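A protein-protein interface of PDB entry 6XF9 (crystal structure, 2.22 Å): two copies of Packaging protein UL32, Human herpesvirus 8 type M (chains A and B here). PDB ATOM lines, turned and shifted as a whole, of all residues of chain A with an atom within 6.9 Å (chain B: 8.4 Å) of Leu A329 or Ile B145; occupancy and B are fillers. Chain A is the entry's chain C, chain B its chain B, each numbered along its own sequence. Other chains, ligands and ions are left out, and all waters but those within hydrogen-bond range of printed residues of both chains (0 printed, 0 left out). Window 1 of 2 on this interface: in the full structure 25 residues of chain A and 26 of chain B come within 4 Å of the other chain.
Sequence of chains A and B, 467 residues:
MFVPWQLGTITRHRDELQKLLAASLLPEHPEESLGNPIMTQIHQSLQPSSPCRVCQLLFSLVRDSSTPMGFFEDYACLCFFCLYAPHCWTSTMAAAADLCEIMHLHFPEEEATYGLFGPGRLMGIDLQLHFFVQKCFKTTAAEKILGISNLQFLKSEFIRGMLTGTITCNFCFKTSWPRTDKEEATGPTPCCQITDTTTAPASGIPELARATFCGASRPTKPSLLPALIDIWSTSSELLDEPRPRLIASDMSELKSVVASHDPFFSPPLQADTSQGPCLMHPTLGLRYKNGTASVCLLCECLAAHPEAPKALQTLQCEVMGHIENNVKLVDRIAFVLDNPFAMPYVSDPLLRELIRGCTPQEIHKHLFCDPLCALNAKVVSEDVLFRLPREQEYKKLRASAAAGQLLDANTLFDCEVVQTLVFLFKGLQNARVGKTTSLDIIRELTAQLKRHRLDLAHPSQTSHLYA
No position is printed for both chains.
Of the 18 printed residues of chain A, 10 touch a printed residue of chain B.
Hydrophobic or aromatic side chains of chain B within 4 Å of the printed part of chain A: Ala B142, Ile B145, Leu B146 and Ile B148.
Among the printed residues, pairs that only touch across the chains: Met A320 with Ala B142, Asn A325 with Lys B138, Asn A326 with Thr B140, Asn A326 with Ile B148, Leu A329 with Ile B145, Leu A329 with Leu B146, Arg A332 with Ile B145, Ala A334 with Gln B56, Phe A335 with Gln B56 and Ala A457 with Leu B146.
OG1 of Thr B140 is in hydrogen-bond range of O of Asn A325 (3.3 Å).
The side-chain amide nitrogen (NE2) of Gln B56 sits at hydrogen-bond distance from the side-chain carboxylate (OD1) of Asp A331.
The backbone carbonyl oxygen of Ser B50 is in hydrogen-bond range of the side-chain amino group of Lys A328 (2.8 Å).
The side-chain amino group (NZ) of Lys A328 is in hydrogen-bond range of the backbone carbonyl oxygen (O) of Pro B48 (3.1 Å).
ND2 of Asn A326 sits close to NE2 of Gln B152 (3.4 Å).
O of Lys B138 is in hydrogen-bond range of N of Asn A326 (2.9 Å).
Leu A329 touches just these residues of chain B: Ile B145 (3.8 Å) and Leu B146 (3.7 Å).
Of the printed residues of chain B, Arg A332 touches Ile B145 (3.9 Å).
Of the printed residues of chain A, Lys B138 touches Asn A325 and Asn A326.
Of chain A, only Leu A329 and Arg A332 come within 4 Å of Ile B145.
Of the printed residues of chain A, Ile B148 touches Asn A326.
The nearest residue of chain B that does not touch Leu A329 is Ser B149 (5.1 Å).
The nearest residue of chain A that does not touch Ile B145 is Asn A326 (4.4 Å).
The nearest printed residue of chain B that does not touch Asn A326 is Ile B145 (4.4 Å).
The backbone carbonyl oxygen of Asn A325 sits at hydrogen-bond distance from the guanidinium group of Arg A332 (2.9 Å).
O of Val A319 lies within hydrogen-bond range of NH1 of Arg A332 (2.7 Å).
The side-chain hydroxyl (OG) of Ser B149 is in hydrogen-bond range of the backbone carbonyl oxygen (O) of Leu B146 (2.7 Å).
The backbone carbonyl oxygen (O) of Phe A368 sits at hydrogen-bond distance from the backbone NH (N) of Ala A457 (3.1 Å).
O of Val A327 is in hydrogen-bond range of NE of Arg A332 (3.0 Å).
ND2 of Asn B150 lies within hydrogen-bond range of O of Leu B146, 3.4 Å away.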
ATOM      1  N   VAL A 319     -18.800 -14.952   5.734  1.00  0.00           N
ATOM      2  CA  VAL A 319     -19.098 -14.287   4.470  1.00  0.00           C
ATOM      3  C   VAL A 319     -18.036 -14.606   3.431  1.00  0.00           C
ATOM      4  O   VAL A 319     -18.353 -14.908   2.278  1.00  0.00           O
ATOM      5  CB  VAL A 319     -19.203 -12.772   4.703  1.00  0.00           C
ATOM      6  CG1 VAL A 319     -19.139 -12.011   3.393  1.00  0.00           C
ATOM      7  CG2 VAL A 319     -20.491 -12.456   5.407  1.00  0.00           C
ATOM      8  N   MET A 320     -16.759 -14.544   3.828  1.00  0.00           N
ATOM      9  CA  MET A 320     -15.648 -14.801   2.906  1.00  0.00           C
ATOM     10  C   MET A 320     -15.511 -16.280   2.549  1.00  0.00           C
ATOM     11  O   MET A 320     -15.285 -16.624   1.385  1.00  0.00           O
ATOM     12  CB  MET A 320     -14.346 -14.308   3.534  1.00  0.00           C
ATOM     13  CG  MET A 320     -14.288 -12.818   3.718  1.00  0.00           C
ATOM     14  SD  MET A 320     -14.535 -12.025   2.130  1.00  0.00           S
ATOM     15  CE  MET A 320     -12.814 -11.725   1.674  1.00  0.00           C
ATOM     16  N   ASN A 325     -18.095 -19.356  -4.685  1.00  0.00           N
ATOM     17  CA  ASN A 325     -18.408 -18.681  -5.936  1.00  0.00           C
ATOM     18  C   ASN A 325     -18.013 -17.204  -5.906  1.00  0.00           C
ATOM     19  O   ASN A 325     -17.576 -16.639  -4.895  1.00  0.00           O
ATOM     20  CB  ASN A 325     -19.918 -18.622  -6.212  1.00  0.00           C
ATOM     21  CG  ASN A 325     -20.545 -19.939  -6.494  1.00  0.00           C
ATOM     22  OD1 ASN A 325     -21.604 -20.262  -5.942  1.00  0.00           O
ATOM     23  ND2 ASN A 325     -19.932 -20.706  -7.385  1.00  0.00           N
ATOM     24  N   ASN A 326     -18.249 -16.566  -7.047  1.00  0.00           N
ATOM     25  CA  ASN A 326     -18.125 -15.134  -7.266  1.00  0.00           C
ATOM     26  C   ASN A 326     -19.402 -14.417  -6.891  1.00  0.00           C
ATOM     27  O   ASN A 326     -19.873 -13.551  -7.640  1.00  0.00           O
ATOM     28  CB  ASN A 326     -17.772 -14.871  -8.727  1.00  0.00           C
ATOM     29  CG  ASN A 326     -17.172 -13.507  -8.947  1.00  0.00           C
ATOM     30  OD1 ASN A 326     -16.674 -12.876  -8.014  1.00  0.00           O
ATOM     31  ND2 ASN A 326     -17.251 -13.020 -10.187  1.00  0.00           N
ATOM     32  N   VAL A 327     -20.008 -14.759  -5.763  1.00  0.00           N
ATOM     33  CA  VAL A 327     -21.179 -14.018  -5.304  1.00  0.00           C
ATOM     34  C   VAL A 327     -20.710 -12.723  -4.649  1.00  0.00           C
ATOM     35  O   VAL A 327     -19.753 -12.716  -3.860  1.00  0.00           O
ATOM     36  CB  VAL A 327     -22.006 -14.877  -4.331  1.00  0.00           C
ATOM     37  CG1 VAL A 327     -23.214 -14.160  -3.911  1.00  0.00           C
ATOM     38  CG2 VAL A 327     -22.396 -16.192  -4.974  1.00  0.00           C
ATOM     39  N   LYS A 328     -21.382 -11.618  -4.964  1.00  0.00           N
ATOM     40  CA  LYS A 328     -20.946 -10.330  -4.449  1.00  0.00           C
ATOM     41  C   LYS A 328     -21.172 -10.261  -2.946  1.00  0.00           C
ATOM     42  O   LYS A 328     -22.034 -10.941  -2.388  1.00  0.00           O
ATOM     43  CB  LYS A 328     -21.677  -9.203  -5.170  1.00  0.00           C
ATOM     44  CG  LYS A 328     -23.119  -9.005  -4.774  1.00  0.00           C
ATOM     45  CD  LYS A 328     -23.885  -8.247  -5.872  1.00  0.00           C
ATOM     46  CE  LYS A 328     -23.637  -6.757  -5.882  1.00  0.00           C
ATOM     47  NZ  LYS A 328     -24.344  -6.185  -7.052  1.00  0.00           N
ATOM     48  N   LEU A 329     -20.393  -9.411  -2.285  1.00  0.00           N
ATOM     49  CA  LEU A 329     -20.386  -9.411  -0.826  1.00  0.00           C
ATOM     50  C   LEU A 329     -21.774  -9.146  -0.240  1.00  0.00           C
ATOM     51  O   LEU A 329     -22.133  -9.737   0.785  1.00  0.00           O
ATOM     52  CB  LEU A 329     -19.369  -8.394  -0.320  1.00  0.00           C
ATOM     53  CG  LEU A 329     -17.946  -8.863  -0.582  1.00  0.00           C
ATOM     54  CD1 LEU A 329     -16.968  -7.725  -0.449  1.00  0.00           C
ATOM     55  CD2 LEU A 329     -17.634  -9.925   0.443  1.00  0.00           C
ATOM     56  N   VAL A 330     -22.585  -8.287  -0.868  1.00  0.00           N
ATOM     57  CA  VAL A 330     -23.863  -8.008  -0.208  1.00  0.00           C
ATOM     58  C   VAL A 330     -24.777  -9.218  -0.320  1.00  0.00           C
ATOM     59  O   VAL A 330     -25.546  -9.521   0.610  1.00  0.00           O
ATOM     60  CB  VAL A 330     -24.553  -6.734  -0.750  1.00  0.00           C
ATOM     61  CG1 VAL A 330     -23.783  -5.503  -0.346  1.00  0.00           C
ATOM     62  CG2 VAL A 330     -24.749  -6.781  -2.243  1.00  0.00           C
ATOM     63  N   ASP A 331     -24.655  -9.982  -1.410  1.00  0.00           N
ATOM     64  CA  ASP A 331     -25.411 -11.221  -1.522  1.00  0.00           C
ATOM     65  C   ASP A 331     -24.854 -12.289  -0.599  1.00  0.00           C
ATOM     66  O   ASP A 331     -25.620 -13.064  -0.020  1.00  0.00           O
ATOM     67  CB  ASP A 331     -25.392 -11.729  -2.948  1.00  0.00           C
ATOM     68  CG  ASP A 331     -26.283 -10.947  -3.850  1.00  0.00           C
ATOM     69  OD1 ASP A 331     -27.304 -10.407  -3.346  1.00  0.00           O
ATOM     70  OD2 ASP A 331     -25.959 -10.895  -5.064  1.00  0.00           O
ATOM     71  N   ARG A 332     -23.531 -12.377  -0.465  1.00  0.00           N
ATOM     72  CA  ARG A 332     -22.977 -13.344   0.482  1.00  0.00           C
ATOM     73  C   ARG A 332     -23.515 -13.099   1.886  1.00  0.00           C
ATOM     74  O   ARG A 332     -23.881 -14.040   2.600  1.00  0.00           O
ATOM     75  CB  ARG A 332     -21.453 -13.266   0.490  1.00  0.00           C
ATOM     76  CG  ARG A 332     -20.748 -13.827  -0.722  1.00  0.00           C
ATOM     77  CD  ARG A 332     -19.272 -13.598  -0.516  1.00  0.00           C
ATOM     78  NE  ARG A 332     -18.444 -14.157  -1.572  1.00  0.00           N
ATOM     79  CZ  ARG A 332     -17.546 -15.115  -1.359  1.00  0.00           C
ATOM     80  NH1 ARG A 332     -17.367 -15.594  -0.138  1.00  0.00           N
ATOM     81  NH2 ARG A 332     -16.804 -15.581  -2.356  1.00  0.00           N
ATOM     82  N   ILE A 333     -23.569 -11.832   2.292  1.00  0.00           N
ATOM     83  CA  ILE A 333     -24.107 -11.464   3.598  1.00  0.00           C
ATOM     84  C   ILE A 333     -25.576 -11.860   3.702  1.00  0.00           C
ATOM     85  O   ILE A 333     -26.023 -12.388   4.729  1.00  0.00           O
ATOM     86  CB  ILE A 333     -23.919  -9.952   3.817  1.00  0.00           C
ATOM     87  CG1 ILE A 333     -22.436  -9.599   3.905  1.00  0.00           C
ATOM     88  CG2 ILE A 333     -24.668  -9.494   5.054  1.00  0.00           C
ATOM     89  CD1 ILE A 333     -22.165  -8.162   3.590  1.00  0.00           C
ATOM     90  N   ALA A 334     -26.356 -11.586   2.651  1.00  0.00           N
ATOM     91  CA  ALA A 334     -27.770 -11.945   2.679  1.00  0.00           C
ATOM     92  C   ALA A 334     -27.960 -13.454   2.804  1.00  0.00           C
ATOM     93  O   ALA A 334     -28.867 -13.911   3.509  1.00  0.00           O
ATOM     94  CB  ALA A 334     -28.472 -11.409   1.436  1.00  0.00           C
ATOM     95  N   PHE A 335     -27.135 -14.247   2.115  1.00  0.00           N
ATOM     96  CA  PHE A 335     -27.258 -15.700   2.219  1.00  0.00           C
ATOM     97  C   PHE A 335     -26.940 -16.172   3.632  1.00  0.00           C
ATOM     98  O   PHE A 335     -27.692 -16.954   4.217  1.00  0.00           O
ATOM     99  CB  PHE A 335     -26.339 -16.416   1.215  1.00  0.00           C
ATOM    100  CG  PHE A 335     -26.749 -16.245  -0.250  1.00  0.00           C
ATOM    101  CD1 PHE A 335     -27.819 -15.425  -0.616  1.00  0.00           C
ATOM    102  CD2 PHE A 335     -26.076 -16.943  -1.254  1.00  0.00           C
ATOM    103  CE1 PHE A 335     -28.175 -15.283  -1.944  1.00  0.00           C
ATOM    104  CE2 PHE A 335     -26.440 -16.811  -2.577  1.00  0.00           C
ATOM    105  CZ  PHE A 335     -27.488 -15.982  -2.922  1.00  0.00           C
ATOM    106  N   PRO A 360     -28.029  -5.618   4.189  1.00  0.00           N
ATOM    107  CA  PRO A 360     -26.717  -6.080   3.704  1.00  0.00           C
ATOM    108  C   PRO A 360     -25.753  -4.948   3.384  1.00  0.00           C
ATOM    109  O   PRO A 360     -24.533  -5.137   3.478  1.00  0.00           O
ATOM    110  CB  PRO A 360     -27.065  -6.873   2.441  1.00  0.00           C
ATOM    111  CG  PRO A 360     -28.528  -7.107   2.512  1.00  0.00           C
ATOM    112  CD  PRO A 360     -29.109  -5.962   3.253  1.00  0.00           C
ATOM    113  N   HIS A 364     -21.996  -4.843   4.749  1.00  0.00           N
ATOM    114  CA  HIS A 364     -20.933  -4.674   3.769  1.00  0.00           C
ATOM    115  C   HIS A 364     -20.076  -3.470   4.135  1.00  0.00           C
ATOM    116  O   HIS A 364     -18.850  -3.570   4.221  1.00  0.00           O
ATOM    117  CB  HIS A 364     -21.531  -4.485   2.384  1.00  0.00           C
ATOM    118  CG  HIS A 364     -20.509  -4.364   1.301  1.00  0.00           C
ATOM    119  ND1 HIS A 364     -20.677  -3.543   0.209  1.00  0.00           N
ATOM    120  CD2 HIS A 364     -19.327  -4.997   1.119  1.00  0.00           C
ATOM    121  CE1 HIS A 364     -19.629  -3.657  -0.588  1.00  0.00           C
ATOM    122  NE2 HIS A 364     -18.799  -4.540  -0.065  1.00  0.00           N
ATOM    123  N   PHE A 368     -16.318  -4.491   5.193  1.00  0.00           N
ATOM    124  CA  PHE A 368     -15.457  -4.384   4.072  1.00  0.00           C
ATOM    125  C   PHE A 368     -15.157  -3.050   3.439  1.00  0.00           C
ATOM    126  O   PHE A 368     -14.252  -2.969   2.701  1.00  0.00           O
ATOM    127  CB  PHE A 368     -16.018  -5.261   2.989  1.00  0.00           C
ATOM    128  CG  PHE A 368     -16.265  -6.658   3.414  1.00  0.00           C
ATOM    129  CD1 PHE A 368     -15.249  -7.521   3.546  1.00  0.00           C
ATOM    130  CD2 PHE A 368     -17.529  -7.101   3.654  1.00  0.00           C
ATOM    131  CE1 PHE A 368     -15.459  -8.789   3.937  1.00  0.00           C
ATOM    132  CE2 PHE A 368     -17.749  -8.391   4.037  1.00  0.00           C
ATOM    133  CZ  PHE A 368     -16.712  -9.227   4.182  1.00  0.00           C
ATOM    134  N   CYS A 369     -15.901  -2.015   3.708  1.00  0.00           N
ATOM    135  CA  CYS A 369     -15.670  -0.770   3.034  1.00  0.00           C
ATOM    136  C   CYS A 369     -15.217   0.464   3.811  1.00  0.00           C
ATOM    137  O   CYS A 369     -14.201   0.997   3.513  1.00  0.00           O
ATOM    138  CB  CYS A 369     -16.892  -0.391   2.235  1.00  0.00           C
ATOM    139  SG  CYS A 369     -17.596  -1.599   1.139  1.00  0.00           S
ATOM    140  N   ALA A 457     -12.467  -2.283   0.314  1.00  0.00           N
ATOM    141  CA  ALA A 457     -12.851  -1.814  -1.001  1.00  0.00           C
ATOM    142  C   ALA A 457     -12.195  -0.471  -1.265  1.00  0.00           C
ATOM    143  O   ALA A 457     -11.739   0.210  -0.350  1.00  0.00           O
ATOM    144  CB  ALA A 457     -14.360  -1.678  -1.094  1.00  0.00           C
ATOM    145  N   PRO B  48     -24.461  -0.731  -7.810  1.00  0.00           N
ATOM    146  CA  PRO B  48     -23.435  -1.685  -7.357  1.00  0.00           C
ATOM    147  C   PRO B  48     -23.774  -2.423  -6.063  1.00  0.00           C
ATOM    148  O   PRO B  48     -23.237  -3.521  -5.820  1.00  0.00           O
ATOM    149  CB  PRO B  48     -22.194  -0.800  -7.208  1.00  0.00           C
ATOM    150  CG  PRO B  48     -22.391   0.266  -8.232  1.00  0.00           C
ATOM    151  CD  PRO B  48     -23.872   0.553  -8.222  1.00  0.00           C
ATOM    152  N   SER B  49     -24.644  -1.869  -5.226  1.00  0.00           N
ATOM    153  CA  SER B  49     -25.021  -2.507  -3.971  1.00  0.00           C
ATOM    154  C   SER B  49     -26.400  -3.134  -4.046  1.00  0.00           C
ATOM    155  O   SER B  49     -26.951  -3.495  -3.000  1.00  0.00           O
ATOM    156  CB  SER B  49     -25.003  -1.508  -2.813  1.00  0.00           C
ATOM    157  OG  SER B  49     -23.685  -1.182  -2.412  1.00  0.00           O
ATOM    158  N   SER B  50     -26.973  -3.272  -5.260  1.00  0.00           N
ATOM    159  CA  SER B  50     -28.211  -4.003  -5.425  1.00  0.00           C
ATOM    160  C   SER B  50     -27.911  -5.496  -5.459  1.00  0.00           C
ATOM    161  O   SER B  50     -26.852  -5.915  -5.938  1.00  0.00           O
ATOM    162  CB  SER B  50     -28.907  -3.594  -6.716  1.00  0.00           C
ATOM    163  OG  SER B  50     -29.551  -2.335  -6.585  1.00  0.00           O
ATOM    164  N   GLN B  56     -30.267 -14.519  -6.011  1.00  0.00           N
ATOM    165  CA  GLN B  56     -31.285 -14.560  -4.959  1.00  0.00           C
ATOM    166  C   GLN B  56     -32.341 -15.608  -5.263  1.00  0.00           C
ATOM    167  O   GLN B  56     -32.778 -16.333  -4.361  1.00  0.00           O
ATOM    168  CB  GLN B  56     -31.922 -13.181  -4.763  1.00  0.00           C
ATOM    169  CG  GLN B  56     -30.960 -12.191  -4.124  1.00  0.00           C
ATOM    170  CD  GLN B  56     -30.661 -12.504  -2.667  1.00  0.00           C
ATOM    171  OE1 GLN B  56     -31.268 -13.400  -2.071  1.00  0.00           O
ATOM    172  NE2 GLN B  56     -29.672 -11.813  -2.105  1.00  0.00           N
ATOM    173  N   LYS B 138     -18.342 -18.355 -11.267  1.00  0.00           N
ATOM    174  CA  LYS B 138     -16.935 -18.719 -11.297  1.00  0.00           C
ATOM    175  C   LYS B 138     -16.433 -18.966  -9.888  1.00  0.00           C
ATOM    176  O   LYS B 138     -16.733 -18.203  -8.972  1.00  0.00           O
ATOM    177  CB  LYS B 138     -16.132 -17.621 -11.969  1.00  0.00           C
ATOM    178  CG  LYS B 138     -16.153 -17.730 -13.463  1.00  0.00           C
ATOM    179  CD  LYS B 138     -15.514 -16.507 -14.051  1.00  0.00           C
ATOM    180  CE  LYS B 138     -13.993 -16.525 -13.929  1.00  0.00           C
ATOM    181  NZ  LYS B 138     -13.431 -15.411 -14.783  1.00  0.00           N
ATOM    182  N   THR B 139     -15.649 -20.028  -9.705  1.00  0.00           N
ATOM    183  CA  THR B 139     -15.107 -20.299  -8.382  1.00  0.00           C
ATOM    184  C   THR B 139     -13.903 -19.400  -8.158  1.00  0.00           C
ATOM    185  O   THR B 139     -12.899 -19.497  -8.869  1.00  0.00           O
ATOM    186  CB  THR B 139     -14.769 -21.780  -8.200  1.00  0.00           C
ATOM    187  OG1 THR B 139     -13.739 -22.159  -9.105  1.00  0.00           O
ATOM    188  CG2 THR B 139     -16.029 -22.638  -8.456  1.00  0.00           C
ATOM    189  N   THR B 140     -13.995 -18.530  -7.167  1.00  0.00           N
ATOM    190  CA  THR B 140     -12.985 -17.511  -6.966  1.00  0.00           C
ATOM    191  C   THR B 140     -12.395 -17.621  -5.573  1.00  0.00           C
ATOM    192  O   THR B 140     -13.112 -17.879  -4.601  1.00  0.00           O
ATOM    193  CB  THR B 140     -13.603 -16.114  -7.171  1.00  0.00           C
ATOM    194  OG1 THR B 140     -14.578 -15.866  -6.149  1.00  0.00           O
ATOM    195  CG2 THR B 140     -14.280 -16.009  -8.546  1.00  0.00           C
ATOM    196  N   ALA B 141     -11.088 -17.400  -5.480  1.00  0.00           N
ATOM    197  CA  ALA B 141     -10.448 -17.443  -4.185  1.00  0.00           C
ATOM    198  C   ALA B 141     -10.947 -16.282  -3.351  1.00  0.00           C
ATOM    199  O   ALA B 141     -11.278 -15.218  -3.877  1.00  0.00           O
ATOM    200  CB  ALA B 141      -8.931 -17.365  -4.333  1.00  0.00           C
ATOM    201  N   ALA B 142     -11.012 -16.497  -2.035  1.00  0.00           N
ATOM    202  CA  ALA B 142     -11.499 -15.450  -1.141  1.00  0.00           C
ATOM    203  C   ALA B 142     -10.644 -14.184  -1.232  1.00  0.00           C
ATOM    204  O   ALA B 142     -11.183 -13.068  -1.288  1.00  0.00           O
ATOM    205  CB  ALA B 142     -11.555 -15.983   0.290  1.00  0.00           C
ATOM    206  N   GLU B 143      -9.321 -14.327  -1.313  1.00  0.00           N
ATOM    207  CA  GLU B 143      -8.478 -13.138  -1.314  1.00  0.00           C
ATOM    208  C   GLU B 143      -8.706 -12.255  -2.547  1.00  0.00           C
ATOM    209  O   GLU B 143      -8.251 -11.102  -2.554  1.00  0.00           O
ATOM    210  CB  GLU B 143      -6.988 -13.502  -1.253  1.00  0.00           C
ATOM    211  CG  GLU B 143      -6.461 -14.040  -2.562  1.00  0.00           C
ATOM    212  CD  GLU B 143      -6.465 -15.554  -2.587  1.00  0.00           C
ATOM    213  OE1 GLU B 143      -7.076 -16.166  -1.655  1.00  0.00           O
ATOM    214  OE2 GLU B 143      -5.889 -16.125  -3.556  1.00  0.00           O
ATOM    215  N   LYS B 144      -9.391 -12.751  -3.580  1.00  0.00           N
ATOM    216  CA  LYS B 144      -9.637 -11.979  -4.786  1.00  0.00           C
ATOM    217  C   LYS B 144     -10.945 -11.206  -4.759  1.00  0.00           C
ATOM    218  O   LYS B 144     -11.235 -10.483  -5.724  1.00  0.00           O
ATOM    219  CB  LYS B 144      -9.665 -12.903  -5.993  1.00  0.00           C
ATOM    220  CG  LYS B 144      -8.394 -13.637  -6.260  1.00  0.00           C
ATOM    221  CD  LYS B 144      -7.250 -12.706  -6.599  1.00  0.00           C
ATOM    222  CE  LYS B 144      -6.177 -13.449  -7.417  1.00  0.00           C
ATOM    223  NZ  LYS B 144      -6.393 -14.942  -7.502  1.00  0.00           N
ATOM    224  N   ILE B 145     -11.736 -11.303  -3.690  1.00  0.00           N
ATOM    225  CA  ILE B 145     -13.100 -10.799  -3.788  1.00  0.00           C
ATOM    226  C   ILE B 145     -13.110  -9.280  -3.816  1.00  0.00           C
ATOM    227  O   ILE B 145     -13.685  -8.664  -4.723  1.00  0.00           O
ATOM    228  CB  ILE B 145     -13.958 -11.350  -2.641  1.00  0.00           C
ATOM    229  CG1 ILE B 145     -14.138 -12.842  -2.853  1.00  0.00           C
ATOM    230  CG2 ILE B 145     -15.307 -10.690  -2.651  1.00  0.00           C
ATOM    231  CD1 ILE B 145     -14.256 -13.212  -4.333  1.00  0.00           C
ATOM    232  N   LEU B 146     -12.444  -8.647  -2.852  1.00  0.00           N
ATOM    233  CA  LEU B 146     -12.452  -7.189  -2.802  1.00  0.00           C
ATOM    234  C   LEU B 146     -11.959  -6.613  -4.125  1.00  0.00           C
ATOM    235  O   LEU B 146     -12.621  -5.767  -4.737  1.00  0.00           O
ATOM    236  CB  LEU B 146     -11.597  -6.695  -1.635  1.00  0.00           C
ATOM    237  CG  LEU B 146     -12.287  -6.659  -0.271  1.00  0.00           C
ATOM    238  CD1 LEU B 146     -11.408  -5.910   0.696  1.00  0.00           C
ATOM    239  CD2 LEU B 146     -13.659  -6.034  -0.349  1.00  0.00           C
ATOM    240  N   GLY B 147     -10.824  -7.105  -4.612  1.00  0.00           N
ATOM    241  CA  GLY B 147     -10.340  -6.652  -5.909  1.00  0.00           C
ATOM    242  C   GLY B 147     -11.384  -6.782  -6.999  1.00  0.00           C
ATOM    243  O   GLY B 147     -11.672  -5.820  -7.716  1.00  0.00           O
ATOM    244  N   ILE B 148     -12.028  -7.950  -7.090  1.00  0.00           N
ATOM    245  CA  ILE B 148     -13.039  -8.153  -8.131  1.00  0.00           C
ATOM    246  C   ILE B 148     -14.171  -7.145  -7.971  1.00  0.00           C
ATOM    247  O   ILE B 148     -14.673  -6.579  -8.961  1.00  0.00           O
ATOM    248  CB  ILE B 148     -13.560  -9.604  -8.109  1.00  0.00           C
ATOM    249  CG1 ILE B 148     -12.505 -10.572  -8.672  1.00  0.00           C
ATOM    250  CG2 ILE B 148     -14.859  -9.708  -8.884  1.00  0.00           C
ATOM    251  CD1 ILE B 148     -12.647 -11.990  -8.173  1.00  0.00           C
ATOM    252  N   SER B 149     -14.558  -6.859  -6.723  1.00  0.00           N
ATOM    253  CA  SER B 149     -15.688  -5.962  -6.535  1.00  0.00           C
ATOM    254  C   SER B 149     -15.389  -4.587  -7.113  1.00  0.00           C
ATOM    255  O   SER B 149     -16.249  -3.992  -7.780  1.00  0.00           O
ATOM    256  CB  SER B 149     -16.037  -5.878  -5.060  1.00  0.00           C
ATOM    257  OG  SER B 149     -15.187  -4.972  -4.397  1.00  0.00           O
ATOM    258  N   ASN B 150     -14.133  -4.135  -7.022  1.00  0.00           N
ATOM    259  CA  ASN B 150     -13.805  -2.844  -7.628  1.00  0.00           C
ATOM    260  C   ASN B 150     -14.123  -2.862  -9.116  1.00  0.00           C
ATOM    261  O   ASN B 150     -14.888  -2.021  -9.613  1.00  0.00           O
ATOM    262  CB  ASN B 150     -12.343  -2.502  -7.370  1.00  0.00           C
ATOM    263  CG  ASN B 150     -12.068  -2.345  -5.881  1.00  0.00           C
ATOM    264  OD1 ASN B 150     -12.887  -1.761  -5.126  1.00  0.00           O
ATOM    265  ND2 ASN B 150     -10.955  -2.928  -5.423  1.00  0.00           N
ATOM    266  N   LEU B 151     -13.642  -3.895  -9.818  1.00  0.00           N
ATOM    267  CA  LEU B 151     -13.882  -3.984 -11.253  1.00  0.00           C
ATOM    268  C   LEU B 151     -15.367  -4.104 -11.551  1.00  0.00           C
ATOM    269  O   LEU B 151     -15.879  -3.431 -12.450  1.00  0.00           O
ATOM    270  CB  LEU B 151     -13.107  -5.167 -11.818  1.00  0.00           C
ATOM    271  CG  LEU B 151     -11.594  -5.004 -11.871  1.00  0.00           C
ATOM    272  CD1 LEU B 151     -10.985  -6.250 -12.411  1.00  0.00           C
ATOM    273  CD2 LEU B 151     -11.306  -3.911 -12.833  1.00  0.00           C
ATOM    274  N   GLN B 152     -16.103  -4.859 -10.740  1.00  0.00           N
ATOM    275  CA  GLN B 152     -17.533  -4.957 -11.015  1.00  0.00           C
ATOM    276  C   GLN B 152     -18.210  -3.607 -10.827  1.00  0.00           C
ATOM    277  O   GLN B 152     -19.086  -3.219 -11.621  1.00  0.00           O
ATOM    278  CB  GLN B 152     -18.173  -6.017 -10.122  1.00  0.00           C
ATOM    279  CG  GLN B 152     -17.616  -7.427 -10.356  1.00  0.00           C
ATOM    280  CD  GLN B 152     -18.407  -8.496  -9.619  1.00  0.00           C
ATOM    281  OE1 GLN B 152     -19.319  -8.190  -8.829  1.00  0.00           O
ATOM    282  NE2 GLN B 152     -18.083  -9.760  -9.895  1.00  0.00           N
ATOM    283  N   GLU B 416     -10.636 -10.251 -16.319  1.00  0.00           N
ATOM    284  CA  GLU B 416     -11.622  -9.242 -15.944  1.00  0.00           C
ATOM    285  C   GLU B 416     -11.138  -7.824 -16.222  1.00  0.00           C
ATOM    286  O   GLU B 416     -11.956  -6.936 -16.469  1.00  0.00           O
ATOM    287  CB  GLU B 416     -12.018  -9.381 -14.480  1.00  0.00           C
ATOM    288  CG  GLU B 416     -13.365  -8.729 -14.214  1.00  0.00           C
ATOM    289  CD  GLU B 416     -14.032  -9.249 -12.953  1.00  0.00           C
ATOM    290  OE1 GLU B 416     -13.311  -9.896 -12.169  1.00  0.00           O
ATOM    291  OE2 GLU B 416     -15.269  -9.030 -12.748  1.00  0.00           O
